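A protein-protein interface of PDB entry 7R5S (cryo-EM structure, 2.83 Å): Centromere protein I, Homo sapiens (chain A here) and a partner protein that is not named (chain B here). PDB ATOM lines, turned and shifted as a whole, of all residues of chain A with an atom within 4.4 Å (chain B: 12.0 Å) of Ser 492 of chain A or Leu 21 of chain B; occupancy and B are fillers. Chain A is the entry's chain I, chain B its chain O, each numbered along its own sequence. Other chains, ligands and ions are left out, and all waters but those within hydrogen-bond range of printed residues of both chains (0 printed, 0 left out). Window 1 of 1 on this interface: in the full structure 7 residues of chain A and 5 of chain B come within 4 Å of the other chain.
No residue of chain B comes within 4 Å of Leu 456 of chain A.
Of the printed residues of chain B, Tyr 488 of chain A touches Leu 21 (3.98 Å) and Glu 25 (3.1 Å).
Printed residues of chain B within 4 Å of Cys 491 of chain A: Leu 21.
Ser 492 of chain A touches just these residues of chain B: Leu 18 and Leu 21.
No residue of chain B comes within 4 Å of Leu 494 of chain A.
No residue of chain B comes within 4 Å of Gln 495 of chain A.
Ser 496 of chain A touches none of the printed residues of chain B.
Of the printed residues of chain A, Glu 22 of chain B touches Arg 452.
Hydrophobic or aromatic side chains of chain B within 4 Å of the printed part of chain A: Leu 18 and Leu 21.
Among the printed residues, 6 pairs touch across the chains.
Among the printed residues, no Asp or Glu carboxylate lies within 4 Å of a Lys or Arg side-chain nitrogen of the other chain.
Among the printed residues, merely in contact across the chains: Tyr 488 of chain A with Glu 25 of chain B (3.1 Å), Ser 492 of chain A with Leu 21 of chain B (3.4 Å), Ser 492 of chain A with Leu 18 of chain B (3.7 Å), Cys 491 of chain A with Leu 21 of chain B (3.8 Å), Arg 452 of chain A with Glu 22 of chain B (3.9 Å) and Tyr 488 of chain A with Leu 21 of chain B (3.98 Å).
O of Tyr 488 of chain A sits at hydrogen-bond distance from OG of Ser 492 of chain A (2.6 Å).
The backbone carbonyl oxygen (O) of Ser 492 of chain A sits at hydrogen-bond distance from the side-chain hydroxyl (OG) of Ser 496 of chain A (2.7 Å).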
ATOM      1  N   ARG A 452      36.693  25.397  13.301  1.00  0.00           N
ATOM      2  CA  ARG A 452      35.518  24.828  13.958  1.00  0.00           C
ATOM      3  C   ARG A 452      34.485  24.327  12.955  1.00  0.00           C
ATOM      4  O   ARG A 452      33.987  23.201  13.070  1.00  0.00           O
ATOM      5  CB  ARG A 452      34.898  25.870  14.889  1.00  0.00           C
ATOM      6  CG  ARG A 452      33.615  25.417  15.563  1.00  0.00           C
ATOM      7  CD  ARG A 452      32.994  26.544  16.369  1.00  0.00           C
ATOM      8  NE  ARG A 452      33.892  27.026  17.414  1.00  0.00           N
ATOM      9  CZ  ARG A 452      33.645  28.083  18.179  1.00  0.00           C
ATOM     10  NH1 ARG A 452      32.527  28.776  18.016  1.00  0.00           N
ATOM     11  NH2 ARG A 452      34.517  28.449  19.108  1.00  0.00           N
ATOM     12  N   LEU A 456      33.850  20.344  12.542  1.00  0.00           N
ATOM     13  CA  LEU A 456      32.582  19.798  13.005  1.00  0.00           C
ATOM     14  C   LEU A 456      31.735  19.261  11.860  1.00  0.00           C
ATOM     15  O   LEU A 456      30.896  18.379  12.079  1.00  0.00           O
ATOM     16  CB  LEU A 456      31.814  20.860  13.791  1.00  0.00           C
ATOM     17  CG  LEU A 456      32.424  21.195  15.153  1.00  0.00           C
ATOM     18  CD1 LEU A 456      31.579  22.211  15.892  1.00  0.00           C
ATOM     19  CD2 LEU A 456      32.599  19.935  15.987  1.00  0.00           C
ATOM     20  N   TYR A 488      28.272  29.207  21.931  1.00  0.00           N
ATOM     21  CA  TYR A 488      28.260  28.980  20.491  1.00  0.00           C
ATOM     22  C   TYR A 488      28.900  27.643  20.138  1.00  0.00           C
ATOM     23  O   TYR A 488      28.442  26.953  19.219  1.00  0.00           O
ATOM     24  CB  TYR A 488      28.968  30.131  19.777  1.00  0.00           C
ATOM     25  CG  TYR A 488      28.430  31.491  20.161  1.00  0.00           C
ATOM     26  CD1 TYR A 488      27.248  31.971  19.614  1.00  0.00           C
ATOM     27  CD2 TYR A 488      29.099  32.290  21.077  1.00  0.00           C
ATOM     28  CE1 TYR A 488      26.750  33.210  19.963  1.00  0.00           C
ATOM     29  CE2 TYR A 488      28.609  33.531  21.434  1.00  0.00           C
ATOM     30  CZ  TYR A 488      27.434  33.987  20.874  1.00  0.00           C
ATOM     31  OH  TYR A 488      26.942  35.221  21.225  1.00  0.00           O
ATOM     32  N   PHE A 489      29.951  27.256  20.864  1.00  0.00           N
ATOM     33  CA  PHE A 489      30.527  25.929  20.676  1.00  0.00           C
ATOM     34  C   PHE A 489      29.516  24.841  21.022  1.00  0.00           C
ATOM     35  O   PHE A 489      29.444  23.808  20.345  1.00  0.00           O
ATOM     36  CB  PHE A 489      31.791  25.783  21.524  1.00  0.00           C
ATOM     37  CG  PHE A 489      32.553  24.515  21.270  1.00  0.00           C
ATOM     38  CD1 PHE A 489      33.441  24.425  20.212  1.00  0.00           C
ATOM     39  CD2 PHE A 489      32.386  23.413  22.093  1.00  0.00           C
ATOM     40  CE1 PHE A 489      34.143  23.261  19.976  1.00  0.00           C
ATOM     41  CE2 PHE A 489      33.087  22.246  21.862  1.00  0.00           C
ATOM     42  CZ  PHE A 489      33.966  22.170  20.802  1.00  0.00           C
ATOM     43  N   LYS A 490      28.719  25.065  22.069  1.00  0.00           N
ATOM     44  CA  LYS A 490      27.683  24.106  22.440  1.00  0.00           C
ATOM     45  C   LYS A 490      26.648  23.964  21.330  1.00  0.00           C
ATOM     46  O   LYS A 490      26.259  22.848  20.963  1.00  0.00           O
ATOM     47  CB  LYS A 490      27.017  24.539  23.747  1.00  0.00           C
ATOM     48  CG  LYS A 490      27.972  24.687  24.919  1.00  0.00           C
ATOM     49  CD  LYS A 490      27.218  24.959  26.210  1.00  0.00           C
ATOM     50  CE  LYS A 490      28.129  24.859  27.421  1.00  0.00           C
ATOM     51  NZ  LYS A 490      29.255  25.828  27.355  1.00  0.00           N
ATOM     52  N   CYS A 491      26.190  25.091  20.780  1.00  0.00           N
ATOM     53  CA  CYS A 491      25.221  25.034  19.691  1.00  0.00           C
ATOM     54  C   CYS A 491      25.809  24.346  18.463  1.00  0.00           C
ATOM     55  O   CYS A 491      25.124  23.566  17.787  1.00  0.00           O
ATOM     56  CB  CYS A 491      24.742  26.443  19.343  1.00  0.00           C
ATOM     57  SG  CYS A 491      23.980  27.328  20.721  1.00  0.00           S
ATOM     58  N   SER A 492      27.084  24.609  18.171  1.00  0.00           N
ATOM     59  CA  SER A 492      27.723  23.994  17.014  1.00  0.00           C
ATOM     60  C   SER A 492      27.837  22.483  17.178  1.00  0.00           C
ATOM     61  O   SER A 492      27.556  21.727  16.238  1.00  0.00           O
ATOM     62  CB  SER A 492      29.100  24.616  16.789  1.00  0.00           C
ATOM     63  OG  SER A 492      29.047  26.027  16.911  1.00  0.00           O
ATOM     64  N   VAL A 493      28.238  22.016  18.364  1.00  0.00           N
ATOM     65  CA  VAL A 493      28.359  20.573  18.550  1.00  0.00           C
ATOM     66  C   VAL A 493      26.984  19.918  18.596  1.00  0.00           C
ATOM     67  O   VAL A 493      26.831  18.764  18.181  1.00  0.00           O
ATOM     68  CB  VAL A 493      29.194  20.238  19.801  1.00  0.00           C
ATOM     69  CG1 VAL A 493      30.583  20.847  19.690  1.00  0.00           C
ATOM     70  CG2 VAL A 493      28.500  20.703  21.059  1.00  0.00           C
ATOM     71  N   LEU A 494      25.956  20.634  19.064  1.00  0.00           N
ATOM     72  CA  LEU A 494      24.604  20.085  18.998  1.00  0.00           C
ATOM     73  C   LEU A 494      24.146  19.921  17.554  1.00  0.00           C
ATOM     74  O   LEU A 494      23.557  18.894  17.194  1.00  0.00           O
ATOM     75  CB  LEU A 494      23.635  20.974  19.776  1.00  0.00           C
ATOM     76  CG  LEU A 494      23.678  20.843  21.299  1.00  0.00           C
ATOM     77  CD1 LEU A 494      22.675  21.779  21.948  1.00  0.00           C
ATOM     78  CD2 LEU A 494      23.419  19.405  21.719  1.00  0.00           C
ATOM     79  N   GLN A 495      24.412  20.922  16.710  1.00  0.00           N
ATOM     80  CA  GLN A 495      24.094  20.801  15.289  1.00  0.00           C
ATOM     81  C   GLN A 495      24.849  19.638  14.651  1.00  0.00           C
ATOM     82  O   GLN A 495      24.281  18.875  13.856  1.00  0.00           O
ATOM     83  CB  GLN A 495      24.417  22.113  14.573  1.00  0.00           C
ATOM     84  CG  GLN A 495      24.259  22.062  13.062  1.00  0.00           C
ATOM     85  CD  GLN A 495      22.812  22.123  12.622  1.00  0.00           C
ATOM     86  OE1 GLN A 495      21.928  22.477  13.401  1.00  0.00           O
ATOM     87  NE2 GLN A 495      22.562  21.777  11.365  1.00  0.00           N
ATOM     88  N   SER A 496      26.133  19.489  14.992  1.00  0.00           N
ATOM     89  CA  SER A 496      26.925  18.396  14.435  1.00  0.00           C
ATOM     90  C   SER A 496      26.378  17.039  14.863  1.00  0.00           C
ATOM     91  O   SER A 496      26.312  16.106  14.054  1.00  0.00           O
ATOM     92  CB  SER A 496      28.386  18.543  14.858  1.00  0.00           C
ATOM     93  OG  SER A 496      28.820  19.883  14.725  1.00  0.00           O
ATOM     94  N   PHE A 556      18.653  30.419  23.983  1.00  0.00           N
ATOM     95  CA  PHE A 556      19.383  30.219  22.737  1.00  0.00           C
ATOM     96  C   PHE A 556      19.879  28.785  22.602  1.00  0.00           C
ATOM     97  O   PHE A 556      20.007  28.275  21.483  1.00  0.00           O
ATOM     98  CB  PHE A 556      20.552  31.202  22.655  1.00  0.00           C
ATOM     99  CG  PHE A 556      21.204  31.260  21.303  1.00  0.00           C
ATOM    100  CD1 PHE A 556      20.585  31.908  20.250  1.00  0.00           C
ATOM    101  CD2 PHE A 556      22.440  30.674  21.089  1.00  0.00           C
ATOM    102  CE1 PHE A 556      21.183  31.967  19.006  1.00  0.00           C
ATOM    103  CE2 PHE A 556      23.043  30.728  19.849  1.00  0.00           C
ATOM    104  CZ  PHE A 556      22.413  31.376  18.805  1.00  0.00           C
ATOM    105  N   GLY B  16      25.961  29.159   6.109  1.00  0.00           N
ATOM    106  CA  GLY B  16      25.405  28.105   6.937  1.00  0.00           C
ATOM    107  C   GLY B  16      25.179  28.524   8.376  1.00  0.00           C
ATOM    108  O   GLY B  16      25.355  29.690   8.727  1.00  0.00           O
ATOM    109  N   VAL B  17      24.786  27.564   9.214  1.00  0.00           N
ATOM    110  CA  VAL B  17      24.543  27.863  10.621  1.00  0.00           C
ATOM    111  C   VAL B  17      25.854  27.930  11.394  1.00  0.00           C
ATOM    112  O   VAL B  17      26.016  28.765  12.291  1.00  0.00           O
ATOM    113  CB  VAL B  17      23.580  26.824  11.224  1.00  0.00           C
ATOM    114  CG1 VAL B  17      23.219  27.199  12.653  1.00  0.00           C
ATOM    115  CG2 VAL B  17      22.330  26.703  10.368  1.00  0.00           C
ATOM    116  N   LEU B  18      26.812  27.063  11.057  1.00  0.00           N
ATOM    117  CA  LEU B  18      28.090  27.068  11.760  1.00  0.00           C
ATOM    118  C   LEU B  18      28.884  28.333  11.458  1.00  0.00           C
ATOM    119  O   LEU B  18      29.490  28.924  12.359  1.00  0.00           O
ATOM    120  CB  LEU B  18      28.896  25.824  11.392  1.00  0.00           C
ATOM    121  CG  LEU B  18      28.262  24.479  11.755  1.00  0.00           C
ATOM    122  CD1 LEU B  18      29.169  23.329  11.353  1.00  0.00           C
ATOM    123  CD2 LEU B  18      27.945  24.419  13.239  1.00  0.00           C
ATOM    124  N   ALA B  19      28.886  28.770  10.195  1.00  0.00           N
ATOM    125  CA  ALA B  19      29.565  30.015   9.851  1.00  0.00           C
ATOM    126  C   ALA B  19      28.895  31.209  10.519  1.00  0.00           C
ATOM    127  O   ALA B  19      29.572  32.161  10.927  1.00  0.00           O
ATOM    128  CB  ALA B  19      29.597  30.193   8.335  1.00  0.00           C
ATOM    129  N   HIS B  20      27.568  31.173  10.650  1.00  0.00           N
ATOM    130  CA  HIS B  20      26.870  32.256  11.334  1.00  0.00           C
ATOM    131  C   HIS B  20      27.207  32.278  12.819  1.00  0.00           C
ATOM    132  O   HIS B  20      27.399  33.350  13.401  1.00  0.00           O
ATOM    133  CB  HIS B  20      25.362  32.130  11.124  1.00  0.00           C
ATOM    134  CG  HIS B  20      24.602  33.364  11.490  1.00  0.00           C
ATOM    135  ND1 HIS B  20      24.772  34.563  10.832  1.00  0.00           N
ATOM    136  CD2 HIS B  20      23.672  33.590  12.449  1.00  0.00           C
ATOM    137  CE1 HIS B  20      23.980  35.473  11.367  1.00  0.00           C
ATOM    138  NE2 HIS B  20      23.301  34.909  12.350  1.00  0.00           N
ATOM    139  N   LEU B  21      27.288  31.103  13.449  1.00  0.00           N
ATOM    140  CA  LEU B  21      27.714  31.048  14.843  1.00  0.00           C
ATOM    141  C   LEU B  21      29.140  31.563  14.997  1.00  0.00           C
ATOM    142  O   LEU B  21      29.454  32.268  15.964  1.00  0.00           O
ATOM    143  CB  LEU B  21      27.594  29.621  15.376  1.00  0.00           C
ATOM    144  CG  LEU B  21      26.174  29.090  15.578  1.00  0.00           C
ATOM    145  CD1 LEU B  21      26.200  27.631  16.001  1.00  0.00           C
ATOM    146  CD2 LEU B  21      25.432  29.932  16.602  1.00  0.00           C
ATOM    147  N   GLU B  22      30.012  31.239  14.041  1.00  0.00           N
ATOM    148  CA  GLU B  22      31.380  31.747  14.083  1.00  0.00           C
ATOM    149  C   GLU B  22      31.403  33.269  14.009  1.00  0.00           C
ATOM    150  O   GLU B  22      32.044  33.932  14.834  1.00  0.00           O
ATOM    151  CB  GLU B  22      32.202  31.143  12.944  1.00  0.00           C
ATOM    152  CG  GLU B  22      32.573  29.687  13.144  1.00  0.00           C
ATOM    153  CD  GLU B  22      33.938  29.356  12.575  1.00  0.00           C
ATOM    154  OE1 GLU B  22      34.872  30.164  12.763  1.00  0.00           O
ATOM    155  OE2 GLU B  22      34.077  28.291  11.939  1.00  0.00           O
ATOM    156  N   ARG B  23      30.700  33.842  13.028  1.00  0.00           N
ATOM    157  CA  ARG B  23      30.709  35.292  12.869  1.00  0.00           C
ATOM    158  C   ARG B  23      29.987  36.005  14.006  1.00  0.00           C
ATOM    159  O   ARG B  23      30.258  37.185  14.248  1.00  0.00           O
ATOM    160  CB  ARG B  23      30.098  35.687  11.521  1.00  0.00           C
ATOM    161  CG  ARG B  23      28.597  35.501  11.417  1.00  0.00           C
ATOM    162  CD  ARG B  23      28.065  36.094  10.122  1.00  0.00           C
ATOM    163  NE  ARG B  23      28.686  35.487   8.947  1.00  0.00           N
ATOM    164  CZ  ARG B  23      28.102  34.568   8.184  1.00  0.00           C
ATOM    165  NH1 ARG B  23      26.878  34.148   8.467  1.00  0.00           N
ATOM    166  NH2 ARG B  23      28.744  34.070   7.135  1.00  0.00           N
ATOM    167  N   LEU B  24      29.078  35.322  14.706  1.00  0.00           N
ATOM    168  CA  LEU B  24      28.509  35.896  15.921  1.00  0.00           C
ATOM    169  C   LEU B  24      29.505  35.834  17.072  1.00  0.00           C
ATOM    170  O   LEU B  24      29.521  36.718  17.936  1.00  0.00           O
ATOM    171  CB  LEU B  24      27.216  35.171  16.294  1.00  0.00           C
ATOM    172  CG  LEU B  24      25.971  35.496  15.467  1.00  0.00           C
ATOM    173  CD1 LEU B  24      24.798  34.638  15.912  1.00  0.00           C
ATOM    174  CD2 LEU B  24      25.629  36.972  15.579  1.00  0.00           C
ATOM    175  N   GLU B  25      30.338  34.792  17.102  1.00  0.00           N
ATOM    176  CA  GLU B  25      31.364  34.688  18.133  1.00  0.00           C
ATOM    177  C   GLU B  25      32.461  35.730  17.947  1.00  0.00           C
ATOM    178  O   GLU B  25      32.988  36.253  18.935  1.00  0.00           O
ATOM    179  CB  GLU B  25      31.955  33.277  18.134  1.00  0.00           C
ATOM    180  CG  GLU B  25      33.314  33.149  18.809  1.00  0.00           C
ATOM    181  CD  GLU B  25      33.237  33.261  20.319  1.00  0.00           C
ATOM    182  OE1 GLU B  25      32.123  33.145  20.872  1.00  0.00           O
ATOM    183  OE2 GLU B  25      34.292  33.463  20.955  1.00  0.00           O
ATOM    184  N   THR B  26      32.812  36.048  16.696  1.00  0.00           N
ATOM    185  CA  THR B  26      33.886  37.008  16.452  1.00  0.00           C
ATOM    186  C   THR B  26      33.546  38.385  17.010  1.00  0.00           C
ATOM    187  O   THR B  26      34.400  39.044  17.616  1.00  0.00           O
ATOM    188  CB  THR B  26      34.190  37.107  14.957  1.00  0.00           C
ATOM    189  OG1 THR B  26      33.066  37.673  14.271  1.00  0.00           O
ATOM    190  CG2 THR B  26      34.518  35.740  14.377  1.00  0.00           C
ATOM    191  N   GLN B  27      32.312  38.837  16.818  1.00  0.00           N
ATOM    192  CA  GLN B  27      31.903  40.147  17.313  1.00  0.00           C
ATOM    193  C   GLN B  27      31.801  40.139  18.835  1.00  0.00           C
ATOM    194  O   GLN B  27      31.602  41.181  19.458  1.00  0.00           O
ATOM    195  CB  GLN B  27      30.570  40.569  16.692  1.00  0.00           C
ATOM    196  CG  GLN B  27      29.352  39.869  17.272  1.00  0.00           C
ATOM    197  CD  GLN B  27      28.685  40.671  18.374  1.00  0.00           C
ATOM    198  OE1 GLN B  27      28.905  41.876  18.499  1.00  0.00           O
ATOM    199  NE2 GLN B  27      27.869  40.005  19.181  1.00  0.00           N
